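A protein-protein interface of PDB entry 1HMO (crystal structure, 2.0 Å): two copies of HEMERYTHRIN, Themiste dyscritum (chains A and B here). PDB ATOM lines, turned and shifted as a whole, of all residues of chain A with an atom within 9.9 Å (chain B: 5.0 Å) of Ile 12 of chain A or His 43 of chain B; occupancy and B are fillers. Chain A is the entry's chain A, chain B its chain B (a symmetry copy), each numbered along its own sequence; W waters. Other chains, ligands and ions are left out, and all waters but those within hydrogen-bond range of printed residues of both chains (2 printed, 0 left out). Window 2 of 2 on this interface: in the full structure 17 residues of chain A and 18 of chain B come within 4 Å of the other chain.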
ATOM      1  N   PRO A   5     -11.781  18.032 -19.157  1.00  0.00           N
ATOM      2  CA  PRO A   5     -12.884  17.424 -18.384  1.00  0.00           C
ATOM      3  C   PRO A   5     -13.959  18.466 -18.079  1.00  0.00           C
ATOM      4  O   PRO A   5     -13.742  19.662 -17.912  1.00  0.00           O
ATOM      5  CB  PRO A   5     -12.242  16.827 -17.166  1.00  0.00           C
ATOM      6  CG  PRO A   5     -10.761  16.947 -17.332  1.00  0.00           C
ATOM      7  CD  PRO A   5     -10.510  17.952 -18.437  1.00  0.00           C
ATOM      8  N   CYS A   9     -12.792  18.461 -13.180  1.00  0.00           N
ATOM      9  CA  CYS A   9     -12.327  17.610 -12.130  1.00  0.00           C
ATOM     10  C   CYS A   9     -11.336  16.557 -12.664  1.00  0.00           C
ATOM     11  O   CYS A   9     -11.345  16.163 -13.829  1.00  0.00           O
ATOM     12  CB  CYS A   9     -13.492  16.897 -11.443  1.00  0.00           C
ATOM     13  SG  CYS A   9     -14.551  18.076 -10.548  1.00  0.00           S
ATOM     14  N   TRP A  10     -10.483  16.149 -11.716  1.00  0.00           N
ATOM     15  CA  TRP A  10      -9.441  15.148 -11.959  1.00  0.00           C
ATOM     16  C   TRP A  10     -10.119  13.822 -12.293  1.00  0.00           C
ATOM     17  O   TRP A  10     -11.116  13.475 -11.618  1.00  0.00           O
ATOM     18  CB  TRP A  10      -8.531  15.019 -10.720  1.00  0.00           C
ATOM     19  CG  TRP A  10      -7.360  14.086 -10.791  1.00  0.00           C
ATOM     20  CD1 TRP A  10      -6.051  14.427 -11.063  1.00  0.00           C
ATOM     21  CD2 TRP A  10      -7.360  12.691 -10.477  1.00  0.00           C
ATOM     22  NE1 TRP A  10      -5.252  13.307 -10.951  1.00  0.00           N
ATOM     23  CE2 TRP A  10      -6.025  12.238 -10.612  1.00  0.00           C
ATOM     24  CE3 TRP A  10      -8.344  11.774 -10.123  1.00  0.00           C
ATOM     25  CZ2 TRP A  10      -5.686  10.913 -10.363  1.00  0.00           C
ATOM     26  CZ3 TRP A  10      -8.026  10.471  -9.897  1.00  0.00           C
ATOM     27  CH2 TRP A  10      -6.672  10.040  -9.955  1.00  0.00           C
ATOM     28  N   ASP A  11      -9.504  13.077 -13.175  1.00  0.00           N
ATOM     29  CA  ASP A  11     -10.060  11.695 -13.450  1.00  0.00           C
ATOM     30  C   ASP A  11      -8.827  10.791 -13.451  1.00  0.00           C
ATOM     31  O   ASP A  11      -7.688  11.320 -13.560  1.00  0.00           O
ATOM     32  CB  ASP A  11     -10.957  11.694 -14.655  1.00  0.00           C
ATOM     33  CG  ASP A  11     -10.286  11.879 -15.991  1.00  0.00           C
ATOM     34  OD1 ASP A  11      -9.310  11.200 -16.325  1.00  0.00           O
ATOM     35  OD2 ASP A  11     -10.683  12.781 -16.754  1.00  0.00           O
ATOM     36  N   ILE A  12      -9.045   9.499 -13.449  1.00  0.00           N
ATOM     37  CA  ILE A  12      -7.898   8.561 -13.422  1.00  0.00           C
ATOM     38  C   ILE A  12      -7.071   8.588 -14.680  1.00  0.00           C
ATOM     39  O   ILE A  12      -5.957   7.995 -14.693  1.00  0.00           O
ATOM     40  CB  ILE A  12      -8.388   7.119 -13.023  1.00  0.00           C
ATOM     41  CG1 ILE A  12      -9.285   6.619 -14.158  1.00  0.00           C
ATOM     42  CG2 ILE A  12      -9.054   7.083 -11.626  1.00  0.00           C
ATOM     43  CD1 ILE A  12      -9.608   5.146 -14.292  1.00  0.00           C
ATOM     44  N   SER A  13      -7.488   9.250 -15.745  1.00  0.00           N
ATOM     45  CA  SER A  13      -6.647   9.341 -16.963  1.00  0.00           C
ATOM     46  C   SER A  13      -5.420  10.200 -16.634  1.00  0.00           C
ATOM     47  O   SER A  13      -4.428  10.161 -17.362  1.00  0.00           O
ATOM     48  CB  SER A  13      -7.378   9.851 -18.176  1.00  0.00           C
ATOM     49  OG  SER A  13      -7.565  11.239 -18.270  1.00  0.00           O
ATOM     50  N   PHE A  14      -5.514  10.986 -15.562  1.00  0.00           N
ATOM     51  CA  PHE A  14      -4.423  11.890 -15.149  1.00  0.00           C
ATOM     52  C   PHE A  14      -3.464  11.212 -14.218  1.00  0.00           C
ATOM     53  O   PHE A  14      -2.508  11.846 -13.773  1.00  0.00           O
ATOM     54  CB  PHE A  14      -5.047  13.151 -14.478  1.00  0.00           C
ATOM     55  CG  PHE A  14      -5.588  14.067 -15.554  1.00  0.00           C
ATOM     56  CD1 PHE A  14      -6.937  13.927 -15.902  1.00  0.00           C
ATOM     57  CD2 PHE A  14      -4.765  14.914 -16.245  1.00  0.00           C
ATOM     58  CE1 PHE A  14      -7.452  14.711 -16.922  1.00  0.00           C
ATOM     59  CE2 PHE A  14      -5.250  15.763 -17.247  1.00  0.00           C
ATOM     60  CZ  PHE A  14      -6.622  15.638 -17.578  1.00  0.00           C
ATOM     61  N   ARG A  15      -3.680   9.967 -13.893  1.00  0.00           N
ATOM     62  CA  ARG A  15      -2.791   9.282 -12.954  1.00  0.00           C
ATOM     63  C   ARG A  15      -1.318   9.319 -13.330  1.00  0.00           C
ATOM     64  O   ARG A  15      -0.946   8.955 -14.434  1.00  0.00           O
ATOM     65  CB  ARG A  15      -3.129   7.815 -12.769  1.00  0.00           C
ATOM     66  CG  ARG A  15      -4.034   7.533 -11.608  1.00  0.00           C
ATOM     67  CD  ARG A  15      -4.396   6.078 -11.577  1.00  0.00           C
ATOM     68  NE  ARG A  15      -5.413   5.885 -10.541  1.00  0.00           N
ATOM     69  CZ  ARG A  15      -6.256   4.856 -10.519  1.00  0.00           C
ATOM     70  NH1 ARG A  15      -6.240   3.952 -11.526  1.00  0.00           N
ATOM     71  NH2 ARG A  15      -6.973   4.610  -9.379  1.00  0.00           N
ATOM     72  N   THR A  16      -0.483   9.627 -12.298  1.00  0.00           N
ATOM     73  CA  THR A  16       0.954   9.596 -12.500  1.00  0.00           C
ATOM     74  C   THR A  16       1.540   8.352 -11.823  1.00  0.00           C
ATOM     75  O   THR A  16       2.684   7.966 -12.138  1.00  0.00           O
ATOM     76  CB  THR A  16       1.724  10.880 -12.013  1.00  0.00           C
ATOM     77  OG1 THR A  16       1.567  10.832 -10.549  1.00  0.00           O
ATOM     78  CG2 THR A  16       1.274  12.190 -12.624  1.00  0.00           C
ATOM     79  N   PHE A  17       0.821   7.747 -10.910  1.00  0.00           N
ATOM     80  CA  PHE A  17       1.249   6.588 -10.115  1.00  0.00           C
ATOM     81  C   PHE A  17       2.037   6.968  -8.876  1.00  0.00           C
ATOM     82  O   PHE A  17       2.396   6.124  -8.026  1.00  0.00           O
ATOM     83  CB  PHE A  17       1.934   5.506 -10.994  1.00  0.00           C
ATOM     84  CG  PHE A  17       0.914   5.060 -12.037  1.00  0.00           C
ATOM     85  CD1 PHE A  17      -0.261   4.416 -11.635  1.00  0.00           C
ATOM     86  CD2 PHE A  17       1.101   5.446 -13.362  1.00  0.00           C
ATOM     87  CE1 PHE A  17      -1.236   4.077 -12.563  1.00  0.00           C
ATOM     88  CE2 PHE A  17       0.125   5.106 -14.322  1.00  0.00           C
ATOM     89  CZ  PHE A  17      -1.042   4.429 -13.899  1.00  0.00           C
ATOM     90  N   ASP A  22      -0.634  12.786  -7.348  1.00  0.00           N
ATOM     91  CA  ASP A  22      -2.030  12.695  -7.805  1.00  0.00           C
ATOM     92  C   ASP A  22      -2.946  13.451  -6.835  1.00  0.00           C
ATOM     93  O   ASP A  22      -3.856  14.119  -7.325  1.00  0.00           O
ATOM     94  CB  ASP A  22      -2.523  11.242  -8.009  1.00  0.00           C
ATOM     95  CG  ASP A  22      -1.841  10.530  -9.182  1.00  0.00           C
ATOM     96  OD1 ASP A  22      -1.229  11.175 -10.072  1.00  0.00           O
ATOM     97  OD2 ASP A  22      -1.871   9.290  -9.123  1.00  0.00           O
ATOM     98  N   HIS A  25      -2.591  17.075  -7.427  1.00  0.00           N
ATOM     99  CA  HIS A  25      -3.215  17.495  -8.710  1.00  0.00           C
ATOM    100  C   HIS A  25      -4.707  17.731  -8.560  1.00  0.00           C
ATOM    101  O   HIS A  25      -5.265  18.697  -9.126  1.00  0.00           O
ATOM    102  CB  HIS A  25      -2.942  16.502  -9.854  1.00  0.00           C
ATOM    103  CG  HIS A  25      -1.523  16.587 -10.361  1.00  0.00           C
ATOM    104  ND1 HIS A  25      -0.918  15.539 -11.043  1.00  0.00           N
ATOM    105  CD2 HIS A  25      -0.594  17.554 -10.269  1.00  0.00           C
ATOM    106  CE1 HIS A  25       0.271  15.963 -11.427  1.00  0.00           C
ATOM    107  NE2 HIS A  25       0.548  17.160 -10.943  1.00  0.00           N
ATOM    108  N   LYS A  26      -5.349  16.860  -7.825  1.00  0.00           N
ATOM    109  CA  LYS A  26      -6.788  16.987  -7.538  1.00  0.00           C
ATOM    110  C   LYS A  26      -7.080  18.344  -6.956  1.00  0.00           C
ATOM    111  O   LYS A  26      -8.116  18.969  -7.229  1.00  0.00           O
ATOM    112  CB  LYS A  26      -7.218  15.886  -6.597  1.00  0.00           C
ATOM    113  CG  LYS A  26      -7.233  14.492  -7.220  1.00  0.00           C
ATOM    114  CD  LYS A  26      -7.434  13.417  -6.170  1.00  0.00           C
ATOM    115  CE  LYS A  26      -6.968  12.066  -6.724  1.00  0.00           C
ATOM    116  NZ  LYS A  26      -6.951  11.048  -5.699  1.00  0.00           N
ATOM    117  N   PHE A  29      -7.131  20.952  -9.899  1.00  0.00           N
ATOM    118  CA  PHE A  29      -8.408  20.920 -10.670  1.00  0.00           C
ATOM    119  C   PHE A  29      -9.504  21.689  -9.920  1.00  0.00           C
ATOM    120  O   PHE A  29     -10.251  22.519 -10.490  1.00  0.00           O
ATOM    121  CB  PHE A  29      -8.811  19.466 -10.944  1.00  0.00           C
ATOM    122  CG  PHE A  29      -8.097  18.878 -12.135  1.00  0.00           C
ATOM    123  CD1 PHE A  29      -6.865  18.246 -11.966  1.00  0.00           C
ATOM    124  CD2 PHE A  29      -8.709  18.957 -13.395  1.00  0.00           C
ATOM    125  CE1 PHE A  29      -6.250  17.639 -13.068  1.00  0.00           C
ATOM    126  CE2 PHE A  29      -8.072  18.446 -14.527  1.00  0.00           C
ATOM    127  CZ  PHE A  29      -6.843  17.781 -14.320  1.00  0.00           C
ATOM    128  N   ILE A 102       0.060  18.290 -17.069  1.00  0.00           N
ATOM    129  CA  ILE A 102       0.142  16.977 -16.471  1.00  0.00           C
ATOM    130  C   ILE A 102       0.433  15.908 -17.536  1.00  0.00           C
ATOM    131  O   ILE A 102       1.334  15.085 -17.329  1.00  0.00           O
ATOM    132  CB  ILE A 102      -1.149  16.652 -15.680  1.00  0.00           C
ATOM    133  CG1 ILE A 102      -1.280  17.695 -14.507  1.00  0.00           C
ATOM    134  CG2 ILE A 102      -1.187  15.199 -15.142  1.00  0.00           C
ATOM    135  CD1 ILE A 102      -2.657  17.535 -13.786  1.00  0.00           C
ATOM    136  N   LYS A 103      -0.422  15.916 -18.545  1.00  0.00           N
ATOM    137  CA  LYS A 103      -0.359  14.850 -19.599  1.00  0.00           C
ATOM    138  C   LYS A 103       0.839  14.910 -20.467  1.00  0.00           C
ATOM    139  O   LYS A 103       1.274  13.859 -21.008  1.00  0.00           O
ATOM    140  CB  LYS A 103      -1.703  14.846 -20.345  1.00  0.00           C
ATOM    141  CG  LYS A 103      -2.738  14.095 -19.488  1.00  0.00           C
ATOM    142  CD  LYS A 103      -4.043  13.887 -20.226  1.00  0.00           C
ATOM    143  CE  LYS A 103      -4.896  12.837 -19.530  1.00  0.00           C
ATOM    144  NZ  LYS A 103      -6.279  12.837 -20.048  1.00  0.00           N
ATOM    145  N   PHE A 107       3.928  13.810 -17.120  1.00  0.00           N
ATOM    146  CA  PHE A 107       3.995  12.365 -17.501  1.00  0.00           C
ATOM    147  C   PHE A 107       5.404  11.941 -17.876  1.00  0.00           C
ATOM    148  O   PHE A 107       5.713  10.723 -17.757  1.00  0.00           O
ATOM    149  CB  PHE A 107       2.943  11.978 -18.566  1.00  0.00           C
ATOM    150  CG  PHE A 107       1.575  11.658 -18.059  1.00  0.00           C
ATOM    151  CD1 PHE A 107       0.682  10.982 -18.927  1.00  0.00           C
ATOM    152  CD2 PHE A 107       1.102  11.998 -16.788  1.00  0.00           C
ATOM    153  CE1 PHE A 107      -0.612  10.729 -18.527  1.00  0.00           C
ATOM    154  CE2 PHE A 107      -0.161  11.670 -16.345  1.00  0.00           C
ATOM    155  CZ  PHE A 107      -1.050  11.020 -17.241  1.00  0.00           C
ATOM    156  N   ARG A 110       7.612  10.137 -15.054  1.00  0.00           N
ATOM    157  CA  ARG A 110       7.198   8.793 -14.571  1.00  0.00           C
ATOM    158  C   ARG A 110       8.258   7.729 -14.851  1.00  0.00           C
ATOM    159  O   ARG A 110       8.838   7.607 -15.942  1.00  0.00           O
ATOM    160  CB  ARG A 110       5.844   8.352 -15.139  1.00  0.00           C
ATOM    161  CG  ARG A 110       4.739   9.401 -14.952  1.00  0.00           C
ATOM    162  CD  ARG A 110       3.387   8.744 -15.233  1.00  0.00           C
ATOM    163  NE  ARG A 110       3.253   8.633 -16.656  1.00  0.00           N
ATOM    164  CZ  ARG A 110       2.231   8.147 -17.344  1.00  0.00           C
ATOM    165  NH1 ARG A 110       1.123   7.706 -16.801  1.00  0.00           N
ATOM    166  NH2 ARG A 110       2.468   8.070 -18.665  1.00  0.00           N
ATOM    167  N   GLY B  31     -13.187  11.708  -5.078  1.00  0.00           N
ATOM    168  CA  GLY B  31     -13.373  10.256  -4.972  1.00  0.00           C
ATOM    169  C   GLY B  31     -14.867   9.950  -5.178  1.00  0.00           C
ATOM    170  O   GLY B  31     -15.208   9.053  -5.984  1.00  0.00           O
ATOM    171  N   LEU B  34     -16.037  10.595  -8.850  1.00  0.00           N
ATOM    172  CA  LEU B  34     -15.731   9.509  -9.774  1.00  0.00           C
ATOM    173  C   LEU B  34     -16.719   8.349  -9.683  1.00  0.00           C
ATOM    174  O   LEU B  34     -17.040   7.784 -10.749  1.00  0.00           O
ATOM    175  CB  LEU B  34     -14.308   9.007  -9.538  1.00  0.00           C
ATOM    176  CG  LEU B  34     -13.199  10.043  -9.580  1.00  0.00           C
ATOM    177  CD1 LEU B  34     -11.844   9.335  -9.369  1.00  0.00           C
ATOM    178  CD2 LEU B  34     -13.233  10.810 -10.880  1.00  0.00           C
ATOM    179  N   LEU B  35     -17.045   7.924  -8.501  1.00  0.00           N
ATOM    180  CA  LEU B  35     -17.986   6.823  -8.286  1.00  0.00           C
ATOM    181  C   LEU B  35     -19.335   7.199  -8.909  1.00  0.00           C
ATOM    182  O   LEU B  35     -20.085   6.398  -9.439  1.00  0.00           O
ATOM    183  CB  LEU B  35     -18.110   6.520  -6.817  1.00  0.00           C
ATOM    184  CG  LEU B  35     -17.137   5.572  -6.173  1.00  0.00           C
ATOM    185  CD1 LEU B  35     -17.538   5.455  -4.689  1.00  0.00           C
ATOM    186  CD2 LEU B  35     -17.147   4.177  -6.764  1.00  0.00           C
ATOM    187  N   ALA B  38     -18.821   6.519 -12.678  1.00  0.00           N
ATOM    188  CA  ALA B  38     -18.631   5.123 -13.083  1.00  0.00           C
ATOM    189  C   ALA B  38     -18.386   4.356 -11.806  1.00  0.00           C
ATOM    190  O   ALA B  38     -17.377   4.602 -11.165  1.00  0.00           O
ATOM    191  CB  ALA B  38     -17.482   4.975 -14.056  1.00  0.00           C
ATOM    192  N   ASN B  40     -16.919   1.745 -10.460  1.00  0.00           N
ATOM    193  CA  ASN B  40     -15.992   0.610 -10.773  1.00  0.00           C
ATOM    194  C   ASN B  40     -14.960   0.482  -9.663  1.00  0.00           C
ATOM    195  O   ASN B  40     -14.907   1.272  -8.705  1.00  0.00           O
ATOM    196  CB  ASN B  40     -15.492   0.814 -12.193  1.00  0.00           C
ATOM    197  CG  ASN B  40     -14.665   2.025 -12.468  1.00  0.00           C
ATOM    198  OD1 ASN B  40     -14.598   2.533 -13.616  1.00  0.00           O
ATOM    199  ND2 ASN B  40     -13.928   2.511 -11.470  1.00  0.00           N
ATOM    200  N   ALA B  41     -14.072  -0.489  -9.802  1.00  0.00           N
ATOM    201  CA  ALA B  41     -12.998  -0.741  -8.841  1.00  0.00           C
ATOM    202  C   ALA B  41     -11.926   0.347  -8.833  1.00  0.00           C
ATOM    203  O   ALA B  41     -11.467   0.659  -7.700  1.00  0.00           O
ATOM    204  CB  ALA B  41     -12.366  -2.116  -9.075  1.00  0.00           C
ATOM    205  N   ASP B  42     -11.499   0.921  -9.933  1.00  0.00           N
ATOM    206  CA  ASP B  42     -10.480   1.962  -9.912  1.00  0.00           C
ATOM    207  C   ASP B  42     -10.934   3.151  -9.064  1.00  0.00           C
ATOM    208  O   ASP B  42     -10.193   3.746  -8.296  1.00  0.00           O
ATOM    209  CB  ASP B  42     -10.135   2.427 -11.330  1.00  0.00           C
ATOM    210  CG  ASP B  42      -9.065   1.504 -11.904  1.00  0.00           C
ATOM    211  OD1 ASP B  42      -8.020   1.358 -11.258  1.00  0.00           O
ATOM    212  OD2 ASP B  42      -9.389   0.858 -12.904  1.00  0.00           O
ATOM    213  N   HIS B  43     -12.178   3.508  -9.305  1.00  0.00           N
ATOM    214  CA  HIS B  43     -12.738   4.678  -8.588  1.00  0.00           C
ATOM    215  C   HIS B  43     -12.907   4.449  -7.118  1.00  0.00           C
ATOM    216  O   HIS B  43     -12.738   5.375  -6.288  1.00  0.00           O
ATOM    217  CB  HIS B  43     -14.055   5.117  -9.263  1.00  0.00           C
ATOM    218  CG  HIS B  43     -13.847   5.657 -10.648  1.00  0.00           C
ATOM    219  ND1 HIS B  43     -14.902   5.974 -11.483  1.00  0.00           N
ATOM    220  CD2 HIS B  43     -12.734   5.989 -11.343  1.00  0.00           C
ATOM    221  CE1 HIS B  43     -14.421   6.521 -12.590  1.00  0.00           C
ATOM    222  NE2 HIS B  43     -13.112   6.494 -12.541  1.00  0.00           N
ATOM    223  N   LEU B  44     -13.338   3.254  -6.749  1.00  0.00           N
ATOM    224  CA  LEU B  44     -13.521   2.914  -5.348  1.00  0.00           C
ATOM    225  C   LEU B  44     -12.165   2.776  -4.643  1.00  0.00           C
ATOM    226  O   LEU B  44     -12.097   3.141  -3.451  1.00  0.00           O
ATOM    227  CB  LEU B  44     -14.416   1.688  -5.265  1.00  0.00           C
ATOM    228  CG  LEU B  44     -14.639   1.076  -3.890  1.00  0.00           C
ATOM    229  CD1 LEU B  44     -15.517   2.016  -3.076  1.00  0.00           C
ATOM    230  CD2 LEU B  44     -15.282  -0.312  -4.023  1.00  0.00           C
ATOM    231  N   ASN B  45     -11.128   2.348  -5.296  1.00  0.00           N
ATOM    232  CA  ASN B  45      -9.797   2.159  -4.685  1.00  0.00           C
ATOM    233  C   ASN B  45      -9.238   3.542  -4.337  1.00  0.00           C
ATOM    234  O   ASN B  45      -8.589   3.767  -3.343  1.00  0.00           O
ATOM    235  CB  ASN B  45      -8.886   1.437  -5.652  1.00  0.00           C
ATOM    236  CG  ASN B  45      -9.146  -0.034  -5.821  1.00  0.00           C
ATOM    237  OD1 ASN B  45      -8.669  -0.599  -6.847  1.00  0.00           O
ATOM    238  ND2 ASN B  45      -9.833  -0.679  -4.904  1.00  0.00           N
ATOM    239  N   GLU B  46      -9.450   4.392  -5.339  1.00  0.00           N
ATOM    240  CA  GLU B  46      -9.055   5.787  -5.249  1.00  0.00           C
ATOM    241  C   GLU B  46      -9.738   6.442  -4.067  1.00  0.00           C
ATOM    242  O   GLU B  46      -9.029   7.036  -3.208  1.00  0.00           O
ATOM    243  CB  GLU B  46      -9.369   6.588  -6.505  1.00  0.00           C
ATOM    244  CG  GLU B  46      -8.555   7.864  -6.665  1.00  0.00           C
ATOM    245  CD  GLU B  46      -7.068   7.706  -6.842  1.00  0.00           C
ATOM    246  OE1 GLU B  46      -6.297   8.593  -6.512  1.00  0.00           O
ATOM    247  OE2 GLU B  46      -6.687   6.642  -7.363  1.00  0.00           O
ATOM    248  N   LEU B  47     -11.066   6.343  -3.958  1.00  0.00           N
ATOM    249  CA  LEU B  47     -11.783   6.915  -2.811  1.00  0.00           C
ATOM    250  C   LEU B  47     -11.334   6.213  -1.530  1.00  0.00           C
ATOM    251  O   LEU B  47     -11.068   6.911  -0.526  1.00  0.00           O
ATOM    252  CB  LEU B  47     -13.306   6.907  -3.032  1.00  0.00           C
ATOM    253  CG  LEU B  47     -14.148   7.261  -1.818  1.00  0.00           C
ATOM    254  CD1 LEU B  47     -13.990   8.768  -1.495  1.00  0.00           C
ATOM    255  CD2 LEU B  47     -15.610   6.969  -2.032  1.00  0.00           C
HETATM  256  O   HOH W   1      -9.987  11.097  -5.309  1.00  0.00           O
HETATM  257  O   HOH W   2      -3.763   7.645  -7.951  1.00  0.00           O
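Water W2 lies within hydrogen-bond range of OD2 of Asp 22 of chain A (2.8 Å) and OE1 of Glu 46 of chain B (3.1 Å). Water W1 lies within hydrogen-bond range of the side-chain amino group (NZ) of Lys 26 of chain A (3.1 Å) and the backbone NH (N) of Gly 31 of chain B (3.3 Å).
Leu 34 of chain B touches Trp 10 of chain A (CD2 to O, 3.5 Å). CH2 of Trp 10 of chain A touches OE1 of Glu 46 of chain B, at 3.8 Å. CG2 of Ile 12 of chain A touches CD2 of His 43 of chain B, 3.8 Å away.
ND2 of Asn 40 of chain B lies close to N of Asp 42 of chain B. The backbone carbonyl oxygen (O) of Arg 15 of chain A lies within hydrogen-bond range of the guanidinium group (NH1) of Arg 110 of chain A. The backbone NH (N) of His 43 of chain B lies close to the side-chain amide nitrogen (ND2) of Asn 40 of chain B, 3.0 Å away. O of Ala 38 of chain B sits at hydrogen-bond distance from ND1 of His 43 of chain B. ND1 of His 43 of chain B is in hydrogen-bond range of O of Leu 34 of chain B (2.9 Å).
OE2 of Glu 46 of chain B lies within salt-bridge range of NH2 of Arg 15 of chain A (2.9 Å). OE1 of Glu 46 of chain B is in salt-bridge range of NZ of Lys 26 of chain A (2.7 Å). The side-chain carboxylate (OD1) of Asp 42 of chain B lies within salt-bridge range of the guanidinium group (NH1) of Arg 15 of chain A (3.2 Å).
Of the printed residues of chain B, Trp 10 of chain A touches Leu 34 (3.5 Å) and Glu 46 (3.8 Å). Of chain B, only His 43 comes within 4 Å of Ile 12 of chain A. Of the printed residues of chain B, Arg 15 of chain A touches Asp 42 and Glu 46. Thr 16 of chain A touches none of the printed residues of chain B. Printed residues of chain B within 4 Å of Lys 26 of chain A: Glu 46. Leu 34 of chain B touches one residue of chain A. Leu 35 of chain B touches none of the printed residues of chain A. No residue of chain A comes within 4 Å of Ala 38 of chain B. Asn 40 of chain B touches none of the printed residues of chain A. No residue of chain A comes within 4 Å of Ala 41 of chain B. Of the printed residues of chain A, His 43 of chain B touches Ile 12. Of the printed residues of chain A, Glu 46 of chain B touches Trp 10, Arg 15 and Lys 26. The nearest residue of chain B that does not touch Ile 12 of chain A is Asp 42 of chain B (4.1 Å). The nearest residue of chain A that does not touch His 43 of chain B is Arg 15 of chain A (5.3 Å).
No position is printed for both chains.
Hydrophobic or aromatic side chains of chain A that line the printed part of chain B: Trp 10 and Ile 12. Of the 12 printed residues of chain B, 4 touch a printed residue of chain A. Hydrophobic or aromatic side chains of chain B within 4 Å of the printed part of chain A: Leu 34 and His 43. Among the printed residues, 6 pairs touch across the chains. Among the printed residues, Asp or Glu carboxylates within 4 Å of a Lys or Arg side-chain nitrogen of the other chain: Arg 15 of chain A with Asp 42 of chain B (3.2 Å), Arg 15 of chain A with Glu 46 of chain B (2.9 Å) and Lys 26 of chain A with Glu 46 of chain B (2.7 Å).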
